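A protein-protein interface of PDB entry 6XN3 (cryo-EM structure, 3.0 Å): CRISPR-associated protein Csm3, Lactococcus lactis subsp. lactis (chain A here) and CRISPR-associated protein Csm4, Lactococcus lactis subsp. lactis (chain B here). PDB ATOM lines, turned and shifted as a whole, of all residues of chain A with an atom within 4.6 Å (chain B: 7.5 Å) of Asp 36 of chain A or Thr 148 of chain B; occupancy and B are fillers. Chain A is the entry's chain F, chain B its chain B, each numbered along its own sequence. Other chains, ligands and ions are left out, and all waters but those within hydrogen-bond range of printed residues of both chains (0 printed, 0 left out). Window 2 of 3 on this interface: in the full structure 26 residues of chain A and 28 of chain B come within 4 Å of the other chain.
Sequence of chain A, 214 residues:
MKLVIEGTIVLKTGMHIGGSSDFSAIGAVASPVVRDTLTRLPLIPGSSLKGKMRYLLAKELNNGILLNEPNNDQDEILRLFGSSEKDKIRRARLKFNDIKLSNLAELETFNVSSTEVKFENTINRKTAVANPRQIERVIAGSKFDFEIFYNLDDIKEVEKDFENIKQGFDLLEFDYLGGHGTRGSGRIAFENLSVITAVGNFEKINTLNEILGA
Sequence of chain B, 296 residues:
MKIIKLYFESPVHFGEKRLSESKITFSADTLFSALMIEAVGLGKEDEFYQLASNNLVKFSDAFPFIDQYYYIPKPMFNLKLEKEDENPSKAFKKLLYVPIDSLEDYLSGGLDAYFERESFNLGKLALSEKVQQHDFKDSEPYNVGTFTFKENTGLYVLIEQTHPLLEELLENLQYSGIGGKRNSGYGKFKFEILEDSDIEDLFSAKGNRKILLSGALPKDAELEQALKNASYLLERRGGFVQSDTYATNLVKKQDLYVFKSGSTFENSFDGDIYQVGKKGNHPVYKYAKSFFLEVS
Asp 36 of chain A touches Thr 148 of chain B (OD1 to CG2, 3.8 Å).
OG1 of Thr 37 of chain A touches CB of Ala 126 of chain B (3.7 Å).
CG2 of Thr 37 of chain A touches OG1 of Thr 148 of chain B, 3.5 Å away.
CD1 of Leu 38 of chain A touches CG of Lys 124 of chain B (3.8 Å).
Thr 148 of chain B touches Leu 38 of chain A.
Leu 38 of chain A touches Phe 149 of chain B.
Lys 150 of chain B touches Leu 38 of chain A.
The backbone carbonyl oxygen (O) of Ala 126 of chain B sits at hydrogen-bond distance from the backbone NH (N) of Thr 146 of chain B.
OG1 of Thr 39 of chain A sits at hydrogen-bond distance from OD2 of Asp 36 of chain A.
The backbone NH of Asp 36 of chain A lies within hydrogen-bond range of the backbone carbonyl oxygen of Leu 41 of chain A, at 3.0 Å.
The backbone carbonyl oxygen of Thr 148 of chain B is in hydrogen-bond range of the backbone NH of Lys 124 of chain B, at 3.4 Å.
OD1 of Asp 36 of chain A sits at hydrogen-bond distance from N of Leu 38 of chain A (3.0 Å).
OD2 of Asp 36 of chain A lies within salt-bridge range of NZ of Lys 100 of chain A, at 3.1 Å.
The backbone carbonyl oxygen of Glu 9 of chain B is in hydrogen-bond range of the side-chain amino group of Lys 100 of chain A.
OG1 of Thr 37 of chain A sits at hydrogen-bond distance from NZ of Lys 124 of chain B (3.4 Å).
Of the 18 printed residues of chain B, 6 touch a printed residue of chain A.
Printed residues of chain B that touch a printed residue of chain A: Glu 9, Lys 124, Ala 126, Thr 148, Phe 149 and Lys 150.
Hydrophobic or aromatic side chains of chain B that line the printed part of chain A: Ala 126.
Along chain B the printed residues that touch a printed residue of chain A span positions 9 to 150.
Hydrophobic or aromatic side chains of chain A within 4 Å of the printed part of chain B: Leu 38.
Among the printed residues, 9 pairs touch across the chains.
Asp 36 of chain A touches just one residue of chain B: Thr 148 (3.8 Å).
Of the printed residues of chain B, Leu 38 of chain A touches Lys 124 (3.8 Å), Thr 148 (3.5 Å), Phe 149 (3.4 Å) and Lys 150 (3.7 Å).
His 13 of chain B touches none of the printed residues of chain A.
Gly 123 of chain B touches none of the printed residues of chain A.
Of the printed residues of chain A, Lys 124 of chain B touches Thr 37 (3.4 Å) and Leu 38 (3.8 Å).
The nearest printed residue of chain A that does not touch Glu 9 of chain B is Asp 36 of chain A (6.0 Å).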
ATOM      1  N   ARG A  35      29.950  30.503 -27.447  1.00  0.00           N
ATOM      2  CA  ARG A  35      29.625  29.126 -27.762  1.00  0.00           C
ATOM      3  C   ARG A  35      28.134  28.908 -27.585  1.00  0.00           C
ATOM      4  O   ARG A  35      27.417  29.761 -27.054  1.00  0.00           O
ATOM      5  CB  ARG A  35      30.400  28.146 -26.878  1.00  0.00           C
ATOM      6  CG  ARG A  35      31.856  27.999 -27.221  1.00  0.00           C
ATOM      7  CD  ARG A  35      32.412  26.759 -26.577  1.00  0.00           C
ATOM      8  NE  ARG A  35      33.815  26.569 -26.898  1.00  0.00           N
ATOM      9  CZ  ARG A  35      34.802  27.051 -26.158  1.00  0.00           C
ATOM     10  NH1 ARG A  35      34.523  27.748 -25.067  1.00  0.00           N
ATOM     11  NH2 ARG A  35      36.059  26.837 -26.501  1.00  0.00           N
ATOM     12  N   ASP A  36      27.668  27.757 -28.055  1.00  0.00           N
ATOM     13  CA  ASP A  36      26.358  27.252 -27.682  1.00  0.00           C
ATOM     14  C   ASP A  36      26.408  26.979 -26.187  1.00  0.00           C
ATOM     15  O   ASP A  36      27.423  26.505 -25.673  1.00  0.00           O
ATOM     16  CB  ASP A  36      26.038  25.988 -28.484  1.00  0.00           C
ATOM     17  CG  ASP A  36      24.604  25.475 -28.295  1.00  0.00           C
ATOM     18  OD1 ASP A  36      23.938  25.742 -27.275  1.00  0.00           O
ATOM     19  OD2 ASP A  36      24.132  24.766 -29.207  1.00  0.00           O
ATOM     20  N   THR A  37      25.318  27.285 -25.488  1.00  0.00           N
ATOM     21  CA  THR A  37      25.329  27.151 -24.037  1.00  0.00           C
ATOM     22  C   THR A  37      25.049  25.725 -23.601  1.00  0.00           C
ATOM     23  O   THR A  37      25.139  25.413 -22.410  1.00  0.00           O
ATOM     24  CB  THR A  37      24.307  28.089 -23.411  1.00  0.00           C
ATOM     25  OG1 THR A  37      24.453  28.063 -21.986  1.00  0.00           O
ATOM     26  CG2 THR A  37      22.909  27.657 -23.782  1.00  0.00           C
ATOM     27  N   LEU A  38      24.712  24.852 -24.539  1.00  0.00           N
ATOM     28  CA  LEU A  38      24.254  23.524 -24.174  1.00  0.00           C
ATOM     29  C   LEU A  38      25.038  22.440 -24.893  1.00  0.00           C
ATOM     30  O   LEU A  38      25.167  21.324 -24.385  1.00  0.00           O
ATOM     31  CB  LEU A  38      22.766  23.415 -24.484  1.00  0.00           C
ATOM     32  CG  LEU A  38      21.956  22.372 -23.748  1.00  0.00           C
ATOM     33  CD1 LEU A  38      22.182  22.522 -22.266  1.00  0.00           C
ATOM     34  CD2 LEU A  38      20.532  22.651 -24.076  1.00  0.00           C
ATOM     35  N   THR A  39      25.563  22.757 -26.069  1.00  0.00           N
ATOM     36  CA  THR A  39      26.413  21.849 -26.817  1.00  0.00           C
ATOM     37  C   THR A  39      27.889  22.151 -26.587  1.00  0.00           C
ATOM     38  O   THR A  39      28.714  21.230 -26.645  1.00  0.00           O
ATOM     39  CB  THR A  39      26.040  21.950 -28.304  1.00  0.00           C
ATOM     40  OG1 THR A  39      24.663  21.598 -28.452  1.00  0.00           O
ATOM     41  CG2 THR A  39      26.827  20.981 -29.172  1.00  0.00           C
ATOM     42  N   ARG A  40      28.203  23.400 -26.225  1.00  0.00           N
ATOM     43  CA  ARG A  40      29.564  23.941 -26.127  1.00  0.00           C
ATOM     44  C   ARG A  40      30.320  23.763 -27.439  1.00  0.00           C
ATOM     45  O   ARG A  40      31.477  23.346 -27.478  1.00  0.00           O
ATOM     46  CB  ARG A  40      30.330  23.342 -24.950  1.00  0.00           C
ATOM     47  CG  ARG A  40      29.635  23.534 -23.638  1.00  0.00           C
ATOM     48  CD  ARG A  40      30.144  24.783 -22.962  1.00  0.00           C
ATOM     49  NE  ARG A  40      31.584  24.935 -23.142  1.00  0.00           N
ATOM     50  CZ  ARG A  40      32.498  24.380 -22.354  1.00  0.00           C
ATOM     51  NH1 ARG A  40      32.126  23.634 -21.324  1.00  0.00           N
ATOM     52  NH2 ARG A  40      33.786  24.573 -22.596  1.00  0.00           N
ATOM     53  N   LEU A  41      29.640  24.109 -28.524  1.00  0.00           N
ATOM     54  CA  LEU A  41      30.186  24.073 -29.862  1.00  0.00           C
ATOM     55  C   LEU A  41      30.339  25.521 -30.309  1.00  0.00           C
ATOM     56  O   LEU A  41      29.425  26.327 -30.077  1.00  0.00           O
ATOM     57  CB  LEU A  41      29.245  23.303 -30.783  1.00  0.00           C
ATOM     58  CG  LEU A  41      29.760  22.738 -32.093  1.00  0.00           C
ATOM     59  CD1 LEU A  41      30.504  21.479 -31.789  1.00  0.00           C
ATOM     60  CD2 LEU A  41      28.590  22.429 -32.998  1.00  0.00           C
ATOM     61  N   LEU A  43      30.494  29.092 -32.322  1.00  0.00           N
ATOM     62  CA  LEU A  43      29.284  29.632 -32.910  1.00  0.00           C
ATOM     63  C   LEU A  43      29.517  31.045 -33.414  1.00  0.00           C
ATOM     64  O   LEU A  43      30.267  31.821 -32.820  1.00  0.00           O
ATOM     65  CB  LEU A  43      28.164  29.616 -31.868  1.00  0.00           C
ATOM     66  CG  LEU A  43      26.742  30.063 -32.156  1.00  0.00           C
ATOM     67  CD1 LEU A  43      25.794  29.102 -31.496  1.00  0.00           C
ATOM     68  CD2 LEU A  43      26.527  31.440 -31.596  1.00  0.00           C
ATOM     69  N   LYS A 100      26.077  27.659 -36.294  1.00  0.00           N
ATOM     70  CA  LYS A 100      26.819  26.710 -35.481  1.00  0.00           C
ATOM     71  C   LYS A 100      27.908  26.062 -36.317  1.00  0.00           C
ATOM     72  O   LYS A 100      27.865  26.096 -37.548  1.00  0.00           O
ATOM     73  CB  LYS A 100      25.887  25.646 -34.904  1.00  0.00           C
ATOM     74  CG  LYS A 100      25.070  26.147 -33.736  1.00  0.00           C
ATOM     75  CD  LYS A 100      24.511  25.021 -32.897  1.00  0.00           C
ATOM     76  CE  LYS A 100      23.006  25.157 -32.765  1.00  0.00           C
ATOM     77  NZ  LYS A 100      22.431  24.198 -31.787  1.00  0.00           N
ATOM     78  N   PHE B   8      12.930  23.328 -31.765  1.00  0.00           N
ATOM     79  CA  PHE B   8      13.803  24.478 -31.939  1.00  0.00           C
ATOM     80  C   PHE B   8      15.234  23.994 -32.094  1.00  0.00           C
ATOM     81  O   PHE B   8      15.716  23.214 -31.270  1.00  0.00           O
ATOM     82  CB  PHE B   8      13.703  25.410 -30.734  1.00  0.00           C
ATOM     83  CG  PHE B   8      12.384  26.101 -30.605  1.00  0.00           C
ATOM     84  CD1 PHE B   8      12.128  27.263 -31.294  1.00  0.00           C
ATOM     85  CD2 PHE B   8      11.405  25.592 -29.778  1.00  0.00           C
ATOM     86  CE1 PHE B   8      10.925  27.904 -31.167  1.00  0.00           C
ATOM     87  CE2 PHE B   8      10.200  26.229 -29.645  1.00  0.00           C
ATOM     88  CZ  PHE B   8       9.959  27.385 -30.342  1.00  0.00           C
ATOM     89  N   GLU B   9      15.914  24.442 -33.151  1.00  0.00           N
ATOM     90  CA  GLU B   9      17.327  24.099 -33.277  1.00  0.00           C
ATOM     91  C   GLU B   9      18.231  25.258 -32.897  1.00  0.00           C
ATOM     92  O   GLU B   9      19.457  25.137 -32.981  1.00  0.00           O
ATOM     93  CB  GLU B   9      17.663  23.636 -34.693  1.00  0.00           C
ATOM     94  CG  GLU B   9      17.535  24.687 -35.766  1.00  0.00           C
ATOM     95  CD  GLU B   9      16.219  24.600 -36.487  1.00  0.00           C
ATOM     96  OE1 GLU B   9      15.277  24.002 -35.934  1.00  0.00           O
ATOM     97  OE2 GLU B   9      16.134  25.101 -37.623  1.00  0.00           O
ATOM     98  N   SER B  10      17.656  26.368 -32.480  1.00  0.00           N
ATOM     99  CA  SER B  10      18.374  27.587 -32.146  1.00  0.00           C
ATOM    100  C   SER B  10      17.840  28.089 -30.817  1.00  0.00           C
ATOM    101  O   SER B  10      16.795  27.626 -30.353  1.00  0.00           O
ATOM    102  CB  SER B  10      18.178  28.608 -33.277  1.00  0.00           C
ATOM    103  OG  SER B  10      16.813  28.948 -33.413  1.00  0.00           O
ATOM    104  N   PRO B  11      18.561  28.983 -30.134  1.00  0.00           N
ATOM    105  CA  PRO B  11      18.038  29.523 -28.874  1.00  0.00           C
ATOM    106  C   PRO B  11      16.795  30.363 -29.096  1.00  0.00           C
ATOM    107  O   PRO B  11      16.511  30.821 -30.196  1.00  0.00           O
ATOM    108  CB  PRO B  11      19.189  30.374 -28.340  1.00  0.00           C
ATOM    109  CG  PRO B  11      20.377  29.830 -28.971  1.00  0.00           C
ATOM    110  CD  PRO B  11      19.976  29.352 -30.314  1.00  0.00           C
ATOM    111  N   VAL B  12      16.015  30.534 -28.038  1.00  0.00           N
ATOM    112  CA  VAL B  12      14.800  31.331 -28.094  1.00  0.00           C
ATOM    113  C   VAL B  12      14.923  32.465 -27.094  1.00  0.00           C
ATOM    114  O   VAL B  12      15.718  32.417 -26.159  1.00  0.00           O
ATOM    115  CB  VAL B  12      13.533  30.509 -27.804  1.00  0.00           C
ATOM    116  CG1 VAL B  12      13.442  29.362 -28.741  1.00  0.00           C
ATOM    117  CG2 VAL B  12      13.552  30.000 -26.390  1.00  0.00           C
ATOM    118  N   HIS B  13      14.133  33.505 -27.315  1.00  0.00           N
ATOM    119  CA  HIS B  13      14.009  34.598 -26.355  1.00  0.00           C
ATOM    120  C   HIS B  13      12.520  34.887 -26.234  1.00  0.00           C
ATOM    121  O   HIS B  13      11.940  35.590 -27.058  1.00  0.00           O
ATOM    122  CB  HIS B  13      14.788  35.829 -26.777  1.00  0.00           C
ATOM    123  CG  HIS B  13      14.440  37.053 -25.992  1.00  0.00           C
ATOM    124  ND1 HIS B  13      14.917  37.284 -24.722  1.00  0.00           N
ATOM    125  CD2 HIS B  13      13.647  38.106 -26.292  1.00  0.00           C
ATOM    126  CE1 HIS B  13      14.438  38.429 -24.276  1.00  0.00           C
ATOM    127  NE2 HIS B  13      13.666  38.949 -25.211  1.00  0.00           N
ATOM    128  N   LEU B 122      14.425  20.491 -19.033  1.00  0.00           N
ATOM    129  CA  LEU B 122      14.665  20.783 -20.434  1.00  0.00           C
ATOM    130  C   LEU B 122      15.520  22.037 -20.490  1.00  0.00           C
ATOM    131  O   LEU B 122      15.204  23.038 -19.839  1.00  0.00           O
ATOM    132  CB  LEU B 122      13.360  20.950 -21.222  1.00  0.00           C
ATOM    133  CG  LEU B 122      12.459  22.189 -21.224  1.00  0.00           C
ATOM    134  CD1 LEU B 122      11.488  22.129 -22.375  1.00  0.00           C
ATOM    135  CD2 LEU B 122      11.722  22.355 -19.918  1.00  0.00           C
ATOM    136  N   GLY B 123      16.645  21.938 -21.189  1.00  0.00           N
ATOM    137  CA  GLY B 123      17.528  23.055 -21.451  1.00  0.00           C
ATOM    138  C   GLY B 123      18.091  23.825 -20.276  1.00  0.00           C
ATOM    139  O   GLY B 123      17.993  23.392 -19.127  1.00  0.00           O
ATOM    140  N   LYS B 124      18.682  24.980 -20.566  1.00  0.00           N
ATOM    141  CA  LYS B 124      19.155  25.875 -19.521  1.00  0.00           C
ATOM    142  C   LYS B 124      19.175  27.293 -20.069  1.00  0.00           C
ATOM    143  O   LYS B 124      19.504  27.508 -21.238  1.00  0.00           O
ATOM    144  CB  LYS B 124      20.535  25.451 -18.994  1.00  0.00           C
ATOM    145  CG  LYS B 124      21.702  25.555 -19.954  1.00  0.00           C
ATOM    146  CD  LYS B 124      22.964  25.048 -19.286  1.00  0.00           C
ATOM    147  CE  LYS B 124      23.413  25.998 -18.188  1.00  0.00           C
ATOM    148  NZ  LYS B 124      23.839  27.309 -18.737  1.00  0.00           N
ATOM    149  N   LEU B 125      18.752  28.239 -19.240  1.00  0.00           N
ATOM    150  CA  LEU B 125      18.703  29.628 -19.656  1.00  0.00           C
ATOM    151  C   LEU B 125      20.106  30.194 -19.780  1.00  0.00           C
ATOM    152  O   LEU B 125      20.970  29.951 -18.936  1.00  0.00           O
ATOM    153  CB  LEU B 125      17.907  30.464 -18.657  1.00  0.00           C
ATOM    154  CG  LEU B 125      16.383  30.508 -18.740  1.00  0.00           C
ATOM    155  CD1 LEU B 125      15.736  29.291 -18.109  1.00  0.00           C
ATOM    156  CD2 LEU B 125      15.891  31.774 -18.081  1.00  0.00           C
ATOM    157  N   ALA B 126      20.325  30.967 -20.837  1.00  0.00           N
ATOM    158  CA  ALA B 126      21.597  31.627 -21.055  1.00  0.00           C
ATOM    159  C   ALA B 126      21.349  33.102 -21.289  1.00  0.00           C
ATOM    160  O   ALA B 126      20.252  33.517 -21.656  1.00  0.00           O
ATOM    161  CB  ALA B 126      22.349  31.040 -22.245  1.00  0.00           C
ATOM    162  N   THR B 146      18.450  34.369 -23.162  1.00  0.00           N
ATOM    163  CA  THR B 146      18.052  33.359 -24.130  1.00  0.00           C
ATOM    164  C   THR B 146      17.681  32.080 -23.399  1.00  0.00           C
ATOM    165  O   THR B 146      17.881  31.944 -22.191  1.00  0.00           O
ATOM    166  CB  THR B 146      19.157  33.050 -25.148  1.00  0.00           C
ATOM    167  OG1 THR B 146      20.230  32.365 -24.493  1.00  0.00           O
ATOM    168  CG2 THR B 146      19.695  34.302 -25.801  1.00  0.00           C
ATOM    169  N   PHE B 147      17.138  31.131 -24.153  1.00  0.00           N
ATOM    170  CA  PHE B 147      16.901  29.787 -23.660  1.00  0.00           C
ATOM    171  C   PHE B 147      17.173  28.814 -24.792  1.00  0.00           C
ATOM    172  O   PHE B 147      16.679  28.993 -25.905  1.00  0.00           O
ATOM    173  CB  PHE B 147      15.472  29.612 -23.161  1.00  0.00           C
ATOM    174  CG  PHE B 147      15.189  28.251 -22.620  1.00  0.00           C
ATOM    175  CD1 PHE B 147      15.725  27.848 -21.419  1.00  0.00           C
ATOM    176  CD2 PHE B 147      14.364  27.381 -23.297  1.00  0.00           C
ATOM    177  CE1 PHE B 147      15.457  26.599 -20.912  1.00  0.00           C
ATOM    178  CE2 PHE B 147      14.101  26.133 -22.795  1.00  0.00           C
ATOM    179  CZ  PHE B 147      14.645  25.745 -21.605  1.00  0.00           C
ATOM    180  N   THR B 148      17.956  27.783 -24.509  1.00  0.00           N
ATOM    181  CA  THR B 148      18.292  26.768 -25.493  1.00  0.00           C
ATOM    182  C   THR B 148      17.724  25.437 -25.037  1.00  0.00           C
ATOM    183  O   THR B 148      17.920  25.030 -23.899  1.00  0.00           O
ATOM    184  CB  THR B 148      19.810  26.648 -25.670  1.00  0.00           C
ATOM    185  OG1 THR B 148      20.343  27.905 -26.100  1.00  0.00           O
ATOM    186  CG2 THR B 148      20.159  25.597 -26.697  1.00  0.00           C
ATOM    187  N   PHE B 149      17.019  24.755 -25.929  1.00  0.00           N
ATOM    188  CA  PHE B 149      16.385  23.485 -25.612  1.00  0.00           C
ATOM    189  C   PHE B 149      17.390  22.361 -25.800  1.00  0.00           C
ATOM    190  O   PHE B 149      18.270  22.453 -26.660  1.00  0.00           O
ATOM    191  CB  PHE B 149      15.164  23.243 -26.497  1.00  0.00           C
ATOM    192  CG  PHE B 149      14.051  24.221 -26.282  1.00  0.00           C
ATOM    193  CD1 PHE B 149      14.014  25.416 -26.971  1.00  0.00           C
ATOM    194  CD2 PHE B 149      13.031  23.934 -25.400  1.00  0.00           C
ATOM    195  CE1 PHE B 149      12.989  26.310 -26.771  1.00  0.00           C
ATOM    196  CE2 PHE B 149      12.002  24.823 -25.208  1.00  0.00           C
ATOM    197  CZ  PHE B 149      11.984  26.012 -25.891  1.00  0.00           C
ATOM    198  N   LYS B 150      17.251  21.297 -25.010  1.00  0.00           N
ATOM    199  CA  LYS B 150      18.077  20.113 -25.195  1.00  0.00           C
ATOM    200  C   LYS B 150      17.676  19.374 -26.466  1.00  0.00           C
ATOM    201  O   LYS B 150      16.705  19.720 -27.142  1.00  0.00           O
ATOM    202  CB  LYS B 150      17.976  19.178 -23.991  1.00  0.00           C
ATOM    203  CG  LYS B 150      18.924  19.521 -22.863  1.00  0.00           C
ATOM    204  CD  LYS B 150      18.544  18.822 -21.573  1.00  0.00           C
ATOM    205  CE  LYS B 150      19.375  19.337 -20.411  1.00  0.00           C
ATOM    206  NZ  LYS B 150      18.929  18.767 -19.112  1.00  0.00           N
ATOM    207  N   GLU B 151      18.445  18.335 -26.787  1.00  0.00           N
ATOM    208  CA  GLU B 151      18.382  17.750 -28.120  1.00  0.00           C
ATOM    209  C   GLU B 151      17.099  16.960 -28.349  1.00  0.00           C
ATOM    210  O   GLU B 151      16.596  16.924 -29.478  1.00  0.00           O
ATOM    211  CB  GLU B 151      19.618  16.873 -28.344  1.00  0.00           C
ATOM    212  CG  GLU B 151      19.729  16.220 -29.718  1.00  0.00           C
ATOM    213  CD  GLU B 151      19.905  17.225 -30.848  1.00  0.00           C
ATOM    214  OE1 GLU B 151      20.419  18.336 -30.603  1.00  0.00           O
ATOM    215  OE2 GLU B 151      19.523  16.904 -31.991  1.00  0.00           O
ATOM    216  N   THR B 153      13.978  17.520 -26.866  1.00  0.00           N
ATOM    217  CA  THR B 153      12.883  18.204 -26.189  1.00  0.00           C
ATOM    218  C   THR B 153      12.484  19.424 -27.009  1.00  0.00           C
ATOM    219  O   THR B 153      13.019  19.666 -28.095  1.00  0.00           O
ATOM    220  CB  THR B 153      13.273  18.591 -24.763  1.00  0.00           C
ATOM    221  OG1 THR B 153      12.143  19.171 -24.109  1.00  0.00           O
ATOM    222  CG2 THR B 153      14.373  19.596 -24.778  1.00  0.00           C
